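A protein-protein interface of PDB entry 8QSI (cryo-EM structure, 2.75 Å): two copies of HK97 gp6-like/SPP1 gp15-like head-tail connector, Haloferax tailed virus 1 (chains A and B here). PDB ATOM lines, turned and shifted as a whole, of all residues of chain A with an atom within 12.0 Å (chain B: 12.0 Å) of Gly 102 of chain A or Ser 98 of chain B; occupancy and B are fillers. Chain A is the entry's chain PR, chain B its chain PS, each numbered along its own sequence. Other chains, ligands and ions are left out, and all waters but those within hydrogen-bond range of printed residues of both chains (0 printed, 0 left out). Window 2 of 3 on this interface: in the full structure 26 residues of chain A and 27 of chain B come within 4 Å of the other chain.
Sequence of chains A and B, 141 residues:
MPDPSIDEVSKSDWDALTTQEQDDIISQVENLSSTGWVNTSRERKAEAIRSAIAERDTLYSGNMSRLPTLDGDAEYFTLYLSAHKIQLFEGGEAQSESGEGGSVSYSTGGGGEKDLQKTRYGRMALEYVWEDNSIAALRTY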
ATOM      1  N   GLN A  95       9.966  21.702  32.361  1.00  0.00           N
ATOM      2  CA  GLN A  95       9.583  22.932  31.688  1.00  0.00           C
ATOM      3  C   GLN A  95       8.270  22.761  30.917  1.00  0.00           C
ATOM      4  O   GLN A  95       7.490  23.705  30.827  1.00  0.00           O
ATOM      5  CB  GLN A  95      10.729  23.375  30.788  1.00  0.00           C
ATOM      6  CG  GLN A  95      10.459  24.683  30.059  1.00  0.00           C
ATOM      7  CD  GLN A  95      11.711  25.399  29.605  1.00  0.00           C
ATOM      8  OE1 GLN A  95      12.830  25.039  29.972  1.00  0.00           O
ATOM      9  NE2 GLN A  95      11.529  26.447  28.812  1.00  0.00           N
ATOM     10  N   SER A  96       8.031  21.565  30.363  1.00  0.00           N
ATOM     11  CA  SER A  96       6.796  21.238  29.657  1.00  0.00           C
ATOM     12  C   SER A  96       6.423  19.790  29.948  1.00  0.00           C
ATOM     13  O   SER A  96       7.297  18.939  30.087  1.00  0.00           O
ATOM     14  CB  SER A  96       6.941  21.405  28.173  1.00  0.00           C
ATOM     15  OG  SER A  96       7.252  22.743  27.828  1.00  0.00           O
ATOM     16  N   GLU A  97       5.114  19.517  30.014  1.00  0.00           N
ATOM     17  CA  GLU A  97       4.570  18.180  30.210  1.00  0.00           C
ATOM     18  C   GLU A  97       3.399  17.974  29.245  1.00  0.00           C
ATOM     19  O   GLU A  97       2.655  18.904  28.944  1.00  0.00           O
ATOM     20  CB  GLU A  97       4.139  17.984  31.662  1.00  0.00           C
ATOM     21  CG  GLU A  97       5.263  18.162  32.672  1.00  0.00           C
ATOM     22  CD  GLU A  97       4.846  17.995  34.126  1.00  0.00           C
ATOM     23  OE1 GLU A  97       4.046  18.815  34.622  1.00  0.00           O
ATOM     24  OE2 GLU A  97       5.322  17.032  34.773  1.00  0.00           O
ATOM     25  N   SER A  98       3.220  16.743  28.756  1.00  0.00           N
ATOM     26  CA  SER A  98       2.197  16.458  27.755  1.00  0.00           C
ATOM     27  C   SER A  98       1.761  14.992  27.831  1.00  0.00           C
ATOM     28  O   SER A  98       2.561  14.128  28.190  1.00  0.00           O
ATOM     29  CB  SER A  98       2.733  16.791  26.387  1.00  0.00           C
ATOM     30  OG  SER A  98       1.733  16.643  25.394  1.00  0.00           O
ATOM     31  N   GLY A  99       0.503  14.705  27.459  1.00  0.00           N
ATOM     32  CA  GLY A  99       0.020  13.333  27.401  1.00  0.00           C
ATOM     33  C   GLY A  99      -1.432  13.188  26.947  1.00  0.00           C
ATOM     34  O   GLY A  99      -2.021  14.101  26.365  1.00  0.00           O
ATOM     35  N   GLU A 100      -1.997  12.016  27.257  1.00  0.00           N
ATOM     36  CA  GLU A 100      -3.370  11.632  26.957  1.00  0.00           C
ATOM     37  C   GLU A 100      -4.355  12.656  27.541  1.00  0.00           C
ATOM     38  O   GLU A 100      -5.391  12.945  26.934  1.00  0.00           O
ATOM     39  CB  GLU A 100      -3.584  10.216  27.512  1.00  0.00           C
ATOM     40  CG  GLU A 100      -4.917   9.545  27.156  1.00  0.00           C
ATOM     41  CD  GLU A 100      -5.073   8.050  27.479  1.00  0.00           C
ATOM     42  OE1 GLU A 100      -4.048   7.331  27.513  1.00  0.00           O
ATOM     43  OE2 GLU A 100      -6.226   7.597  27.696  1.00  0.00           O
ATOM     44  N   GLY A 101      -4.013  13.233  28.709  1.00  0.00           N
ATOM     45  CA  GLY A 101      -4.907  14.077  29.508  1.00  0.00           C
ATOM     46  C   GLY A 101      -4.695  15.594  29.388  1.00  0.00           C
ATOM     47  O   GLY A 101      -5.276  16.341  30.180  1.00  0.00           O
ATOM     48  N   GLY A 102      -3.863  16.054  28.428  1.00  0.00           N
ATOM     49  CA  GLY A 102      -3.632  17.473  28.136  1.00  0.00           C
ATOM     50  C   GLY A 102      -2.151  17.867  28.069  1.00  0.00           C
ATOM     51  O   GLY A 102      -1.293  17.010  27.882  1.00  0.00           O
ATOM     52  N   SER A 103      -1.844  19.168  28.220  1.00  0.00           N
ATOM     53  CA  SER A 103      -0.464  19.659  28.216  1.00  0.00           C
ATOM     54  C   SER A 103      -0.297  20.983  28.978  1.00  0.00           C
ATOM     55  O   SER A 103      -1.225  21.783  29.055  1.00  0.00           O
ATOM     56  CB  SER A 103       0.055  19.772  26.808  1.00  0.00           C
ATOM     57  OG  SER A 103       1.388  20.252  26.802  1.00  0.00           O
ATOM     58  N   VAL A 104       0.908  21.226  29.525  1.00  0.00           N
ATOM     59  CA  VAL A 104       1.252  22.448  30.251  1.00  0.00           C
ATOM     60  C   VAL A 104       2.721  22.819  30.014  1.00  0.00           C
ATOM     61  O   VAL A 104       3.562  21.944  29.828  1.00  0.00           O
ATOM     62  CB  VAL A 104       0.944  22.304  31.753  1.00  0.00           C
ATOM     63  CG1 VAL A 104       1.731  21.170  32.379  1.00  0.00           C
ATOM     64  CG2 VAL A 104       1.178  23.589  32.541  1.00  0.00           C
ATOM     65  N   SER A 105       3.025  24.128  30.034  1.00  0.00           N
ATOM     66  CA  SER A 105       4.386  24.645  30.062  1.00  0.00           C
ATOM     67  C   SER A 105       4.529  25.608  31.237  1.00  0.00           C
ATOM     68  O   SER A 105       3.617  26.390  31.502  1.00  0.00           O
ATOM     69  CB  SER A 105       4.718  25.360  28.789  1.00  0.00           C
ATOM     70  OG  SER A 105       4.911  24.432  27.737  1.00  0.00           O
ATOM     71  N   TYR A 106       5.683  25.573  31.914  1.00  0.00           N
ATOM     72  CA  TYR A 106       5.925  26.389  33.091  1.00  0.00           C
ATOM     73  C   TYR A 106       6.967  27.459  32.784  1.00  0.00           C
ATOM     74  O   TYR A 106       7.927  27.224  32.054  1.00  0.00           O
ATOM     75  CB  TYR A 106       6.399  25.511  34.242  1.00  0.00           C
ATOM     76  CG  TYR A 106       5.494  24.355  34.575  1.00  0.00           C
ATOM     77  CD1 TYR A 106       4.447  24.494  35.476  1.00  0.00           C
ATOM     78  CD2 TYR A 106       5.719  23.101  34.032  1.00  0.00           C
ATOM     79  CE1 TYR A 106       3.631  23.419  35.806  1.00  0.00           C
ATOM     80  CE2 TYR A 106       4.925  22.011  34.364  1.00  0.00           C
ATOM     81  CZ  TYR A 106       3.877  22.168  35.259  1.00  0.00           C
ATOM     82  OH  TYR A 106       3.099  21.094  35.607  1.00  0.00           O
ATOM     83  N   GLU B  93       4.690  28.793  37.873  1.00  0.00           N
ATOM     84  CA  GLU B  93       3.664  29.553  37.167  1.00  0.00           C
ATOM     85  C   GLU B  93       3.452  28.951  35.774  1.00  0.00           C
ATOM     86  O   GLU B  93       4.392  28.885  34.983  1.00  0.00           O
ATOM     87  CB  GLU B  93       4.107  31.016  37.115  1.00  0.00           C
ATOM     88  CG  GLU B  93       3.116  31.953  36.460  1.00  0.00           C
ATOM     89  CD  GLU B  93       3.145  33.324  37.111  1.00  0.00           C
ATOM     90  OE1 GLU B  93       2.470  33.494  38.154  1.00  0.00           O
ATOM     91  OE2 GLU B  93       3.884  34.212  36.627  1.00  0.00           O
ATOM     92  N   ALA B  94       2.217  28.526  35.461  1.00  0.00           N
ATOM     93  CA  ALA B  94       1.907  28.000  34.137  1.00  0.00           C
ATOM     94  C   ALA B  94       1.949  29.122  33.096  1.00  0.00           C
ATOM     95  O   ALA B  94       1.356  30.184  33.290  1.00  0.00           O
ATOM     96  CB  ALA B  94       0.574  27.289  34.154  1.00  0.00           C
ATOM     97  N   GLN B  95       2.662  28.871  31.989  1.00  0.00           N
ATOM     98  CA  GLN B  95       2.780  29.801  30.878  1.00  0.00           C
ATOM     99  C   GLN B  95       1.810  29.450  29.746  1.00  0.00           C
ATOM    100  O   GLN B  95       1.296  30.344  29.082  1.00  0.00           O
ATOM    101  CB  GLN B  95       4.234  29.838  30.422  1.00  0.00           C
ATOM    102  CG  GLN B  95       4.473  30.738  29.218  1.00  0.00           C
ATOM    103  CD  GLN B  95       5.900  31.211  29.084  1.00  0.00           C
ATOM    104  OE1 GLN B  95       6.724  31.042  29.984  1.00  0.00           O
ATOM    105  NE2 GLN B  95       6.208  31.825  27.948  1.00  0.00           N
ATOM    106  N   SER B  96       1.561  28.151  29.528  1.00  0.00           N
ATOM    107  CA  SER B  96       0.600  27.671  28.539  1.00  0.00           C
ATOM    108  C   SER B  96      -0.129  26.457  29.104  1.00  0.00           C
ATOM    109  O   SER B  96       0.456  25.663  29.835  1.00  0.00           O
ATOM    110  CB  SER B  96       1.271  27.278  27.254  1.00  0.00           C
ATOM    111  OG  SER B  96       1.943  28.372  26.654  1.00  0.00           O
ATOM    112  N   GLU B  97      -1.409  26.315  28.741  1.00  0.00           N
ATOM    113  CA  GLU B  97      -2.251  25.194  29.140  1.00  0.00           C
ATOM    114  C   GLU B  97      -3.077  24.737  27.933  1.00  0.00           C
ATOM    115  O   GLU B  97      -3.493  25.550  27.113  1.00  0.00           O
ATOM    116  CB  GLU B  97      -3.153  25.595  30.304  1.00  0.00           C
ATOM    117  CG  GLU B  97      -2.396  26.043  31.542  1.00  0.00           C
ATOM    118  CD  GLU B  97      -3.277  26.430  32.718  1.00  0.00           C
ATOM    119  OE1 GLU B  97      -3.980  27.460  32.634  1.00  0.00           O
ATOM    120  OE2 GLU B  97      -3.264  25.691  33.726  1.00  0.00           O
ATOM    121  N   SER B  98      -3.328  23.429  27.820  1.00  0.00           N
ATOM    122  CA  SER B  98      -4.040  22.883  26.669  1.00  0.00           C
ATOM    123  C   SER B  98      -4.757  21.581  27.045  1.00  0.00           C
ATOM    124  O   SER B  98      -4.295  20.851  27.923  1.00  0.00           O
ATOM    125  CB  SER B  98      -3.072  22.658  25.536  1.00  0.00           C
ATOM    126  OG  SER B  98      -3.746  22.222  24.368  1.00  0.00           O
ATOM    127  N   GLY B  99      -5.870  21.272  26.356  1.00  0.00           N
ATOM    128  CA  GLY B  99      -6.576  20.017  26.565  1.00  0.00           C
ATOM    129  C   GLY B  99      -7.785  19.808  25.655  1.00  0.00           C
ATOM    130  O   GLY B  99      -7.935  20.461  24.620  1.00  0.00           O
ATOM    131  N   GLU B 100      -8.658  18.895  26.090  1.00  0.00           N
ATOM    132  CA  GLU B 100      -9.901  18.523  25.426  1.00  0.00           C
ATOM    133  C   GLU B 100     -10.800  19.755  25.235  1.00  0.00           C
ATOM    134  O   GLU B 100     -11.537  19.849  24.248  1.00  0.00           O
ATOM    135  CB  GLU B 100     -10.562  17.424  26.274  1.00  0.00           C
ATOM    136  CG  GLU B 100     -11.797  16.742  25.669  1.00  0.00           C
ATOM    137  CD  GLU B 100     -12.337  15.488  26.376  1.00  0.00           C
ATOM    138  OE1 GLU B 100     -11.534  14.752  26.994  1.00  0.00           O
ATOM    139  OE2 GLU B 100     -13.567  15.241  26.308  1.00  0.00           O
ATOM    140  N   GLY B 101     -10.719  20.719  26.172  1.00  0.00           N
ATOM    141  CA  GLY B 101     -11.638  21.857  26.266  1.00  0.00           C
ATOM    142  C   GLY B 101     -11.102  23.204  25.758  1.00  0.00           C
ATOM    143  O   GLY B 101     -11.759  24.225  25.978  1.00  0.00           O
ATOM    144  N   GLY B 102      -9.919  23.223  25.107  1.00  0.00           N
ATOM    145  CA  GLY B 102      -9.314  24.419  24.511  1.00  0.00           C
ATOM    146  C   GLY B 102      -7.852  24.649  24.913  1.00  0.00           C
ATOM    147  O   GLY B 102      -7.189  23.728  25.382  1.00  0.00           O
ATOM    148  N   SER B 103      -7.343  25.881  24.728  1.00  0.00           N
ATOM    149  CA  SER B 103      -5.969  26.232  25.091  1.00  0.00           C
ATOM    150  C   SER B 103      -5.809  27.724  25.425  1.00  0.00           C
ATOM    151  O   SER B 103      -6.532  28.566  24.901  1.00  0.00           O
ATOM    152  CB  SER B 103      -5.008  25.802  24.013  1.00  0.00           C
ATOM    153  OG  SER B 103      -3.677  26.145  24.357  1.00  0.00           O
ATOM    154  N   VAL B 104      -4.838  28.055  26.293  1.00  0.00           N
ATOM    155  CA  VAL B 104      -4.524  29.426  26.689  1.00  0.00           C
ATOM    156  C   VAL B 104      -3.012  29.586  26.889  1.00  0.00           C
ATOM    157  O   VAL B 104      -2.329  28.633  27.253  1.00  0.00           O
ATOM    158  CB  VAL B 104      -5.315  29.832  27.948  1.00  0.00           C
ATOM    159  CG1 VAL B 104      -5.026  28.925  29.132  1.00  0.00           C
ATOM    160  CG2 VAL B 104      -5.102  31.288  28.342  1.00  0.00           C
ATOM    161  N   SER B 105      -2.482  30.794  26.642  1.00  0.00           N
ATOM    162  CA  SER B 105      -1.121  31.162  27.018  1.00  0.00           C
ATOM    163  C   SER B 105      -1.137  32.506  27.740  1.00  0.00           C
ATOM    164  O   SER B 105      -1.912  33.386  27.374  1.00  0.00           O
ATOM    165  CB  SER B 105      -0.223  31.238  25.825  1.00  0.00           C
ATOM    166  OG  SER B 105      -0.012  29.943  25.293  1.00  0.00           O
ATOM    167  N   TYR B 106      -0.265  32.672  28.744  1.00  0.00           N
ATOM    168  CA  TYR B 106      -0.295  33.847  29.600  1.00  0.00           C
ATOM    169  C   TYR B 106       0.947  34.717  29.415  1.00  0.00           C
ATOM    170  O   TYR B 106       2.070  34.223  29.334  1.00  0.00           O
ATOM    171  CB  TYR B 106      -0.403  33.426  31.061  1.00  0.00           C
ATOM    172  CG  TYR B 106      -1.562  32.525  31.399  1.00  0.00           C
ATOM    173  CD1 TYR B 106      -2.826  33.039  31.653  1.00  0.00           C
ATOM    174  CD2 TYR B 106      -1.383  31.157  31.525  1.00  0.00           C
ATOM    175  CE1 TYR B 106      -3.890  32.212  31.995  1.00  0.00           C
ATOM    176  CE2 TYR B 106      -2.433  30.317  31.871  1.00  0.00           C
ATOM    177  CZ  TYR B 106      -3.691  30.844  32.117  1.00  0.00           C
ATOM    178  OH  TYR B 106      -4.720  30.018  32.486  1.00  0.00           O
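The backbone NH (N) of Ser 98 of chain B lies within hydrogen-bond range of the backbone carbonyl oxygen (O) of Ser 103 of chain A, at 2.9 Å.
The backbone NH (N) of Gln 95 of chain B sits at hydrogen-bond distance from the backbone carbonyl oxygen (O) of Ser 105 of chain A, 2.7 Å away.
N of Ser 105 of chain A is in hydrogen-bond range of O of Ser 96 of chain B, at 3.0 Å.
The side-chain hydroxyl of Ser 105 of chain A is in hydrogen-bond range of the side-chain hydroxyl of Ser 96 of chain A.
The side-chain carboxylate (OE1) of Glu 97 of chain A sits at hydrogen-bond distance from the side-chain hydroxyl (OH) of Tyr 106 of chain A (2.7 Å).
The side-chain hydroxyl (OG) of Ser 105 of chain B lies within hydrogen-bond range of the side-chain hydroxyl (OG) of Ser 96 of chain B, at 2.9 Å.
The side-chain hydroxyl (OG) of Ser 103 of chain B lies within hydrogen-bond range of the backbone carbonyl oxygen (O) of Glu 97 of chain B, 2.8 Å away.
The backbone NH of Glu 97 of chain B is in hydrogen-bond range of the backbone carbonyl oxygen of Val 104 of chain B (2.9 Å).
The side-chain carboxylate of Glu 97 of chain B lies within hydrogen-bond range of the side-chain hydroxyl of Tyr 106 of chain B (2.7 Å).
Among the printed residues, pairs that only touch across the chains: Gly 102 of chain A with Ser 98 of chain B, Ser 103 of chain A with Glu 97 of chain B, Val 104 of chain A with Ser 96 of chain B, Ser 105 of chain A with Ala 94 of chain B and Tyr 106 of chain A with Glu 93 of chain B.
No residue of chain B comes within 4 Å of Ser 98 of chain A.
No residue of chain B comes within 4 Å of Gly 99 of chain A.
Printed residues of chain B within 4 Å of Gly 102 of chain A: Ser 98.
Ser 103 of chain A touches two residues of chain B.
Val 104 of chain A touches just one residue of chain B: Ser 96 (3.3 Å).
Printed residues of chain B within 4 Å of Ser 105 of chain A: Ala 94 (3.5 Å), Gln 95 (2.7 Å) and Ser 96 (3.0 Å).
Printed residues of chain B within 4 Å of Tyr 106 of chain A: Glu 93 (3.5 Å).
Of the printed residues of chain A, Glu 93 of chain B touches Tyr 106.
Printed residues of chain A within 4 Å of Ala 94 of chain B: Ser 105.
Of the printed residues of chain A, Gln 95 of chain B touches Ser 105 (2.7 Å).
Ser 96 of chain B touches two residues of chain A.
Of the printed residues of chain A, Glu 97 of chain B touches Ser 103.
Printed residues of chain A within 4 Å of Ser 98 of chain B: Gly 102 and Ser 103.
No residue of chain A comes within 4 Å of Gly 99 of chain B.
No residue of chain A comes within 4 Å of Gly 101 of chain B.
No residue of chain A comes within 4 Å of Gly 102 of chain B.
No residue of chain A comes within 4 Å of Ser 103 of chain B.
The nearest printed residue of chain A that does not touch Ala 94 of chain B is Val 104 of chain A (4.1 Å).
Hydrophobic or aromatic side chains of chain A within 4 Å of the printed part of chain B: Val 104 and Tyr 106.
Of the 14 printed residues of chain B, 6 touch a printed residue of chain A.
Among the printed residues, 8 pairs touch across the chains.
Gly 102 of chain A touches Ser 98 of chain B, but with the chains exchanged Ser 98 of chain A does not touch Gly 102 of chain B (11.4 Å).
Ser 103 of chain A touches Glu 97 of chain B, but with the chains exchanged Glu 97 of chain A does not touch Ser 103 of chain B (10.7 Å).
Val 104 of chain A touches Ser 96 of chain B, but with the chains exchanged Ser 96 of chain A does not touch Val 104 of chain B (11.3 Å).
Ser 105 of chain A touches Ser 96 of chain B, but with the chains exchanged Ser 96 of chain A does not touch Ser 105 of chain B (10.5 Å).
Of the 8 pairs that touch across the chains among the printed residues, none has its exchanged pair printed and touching as well.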
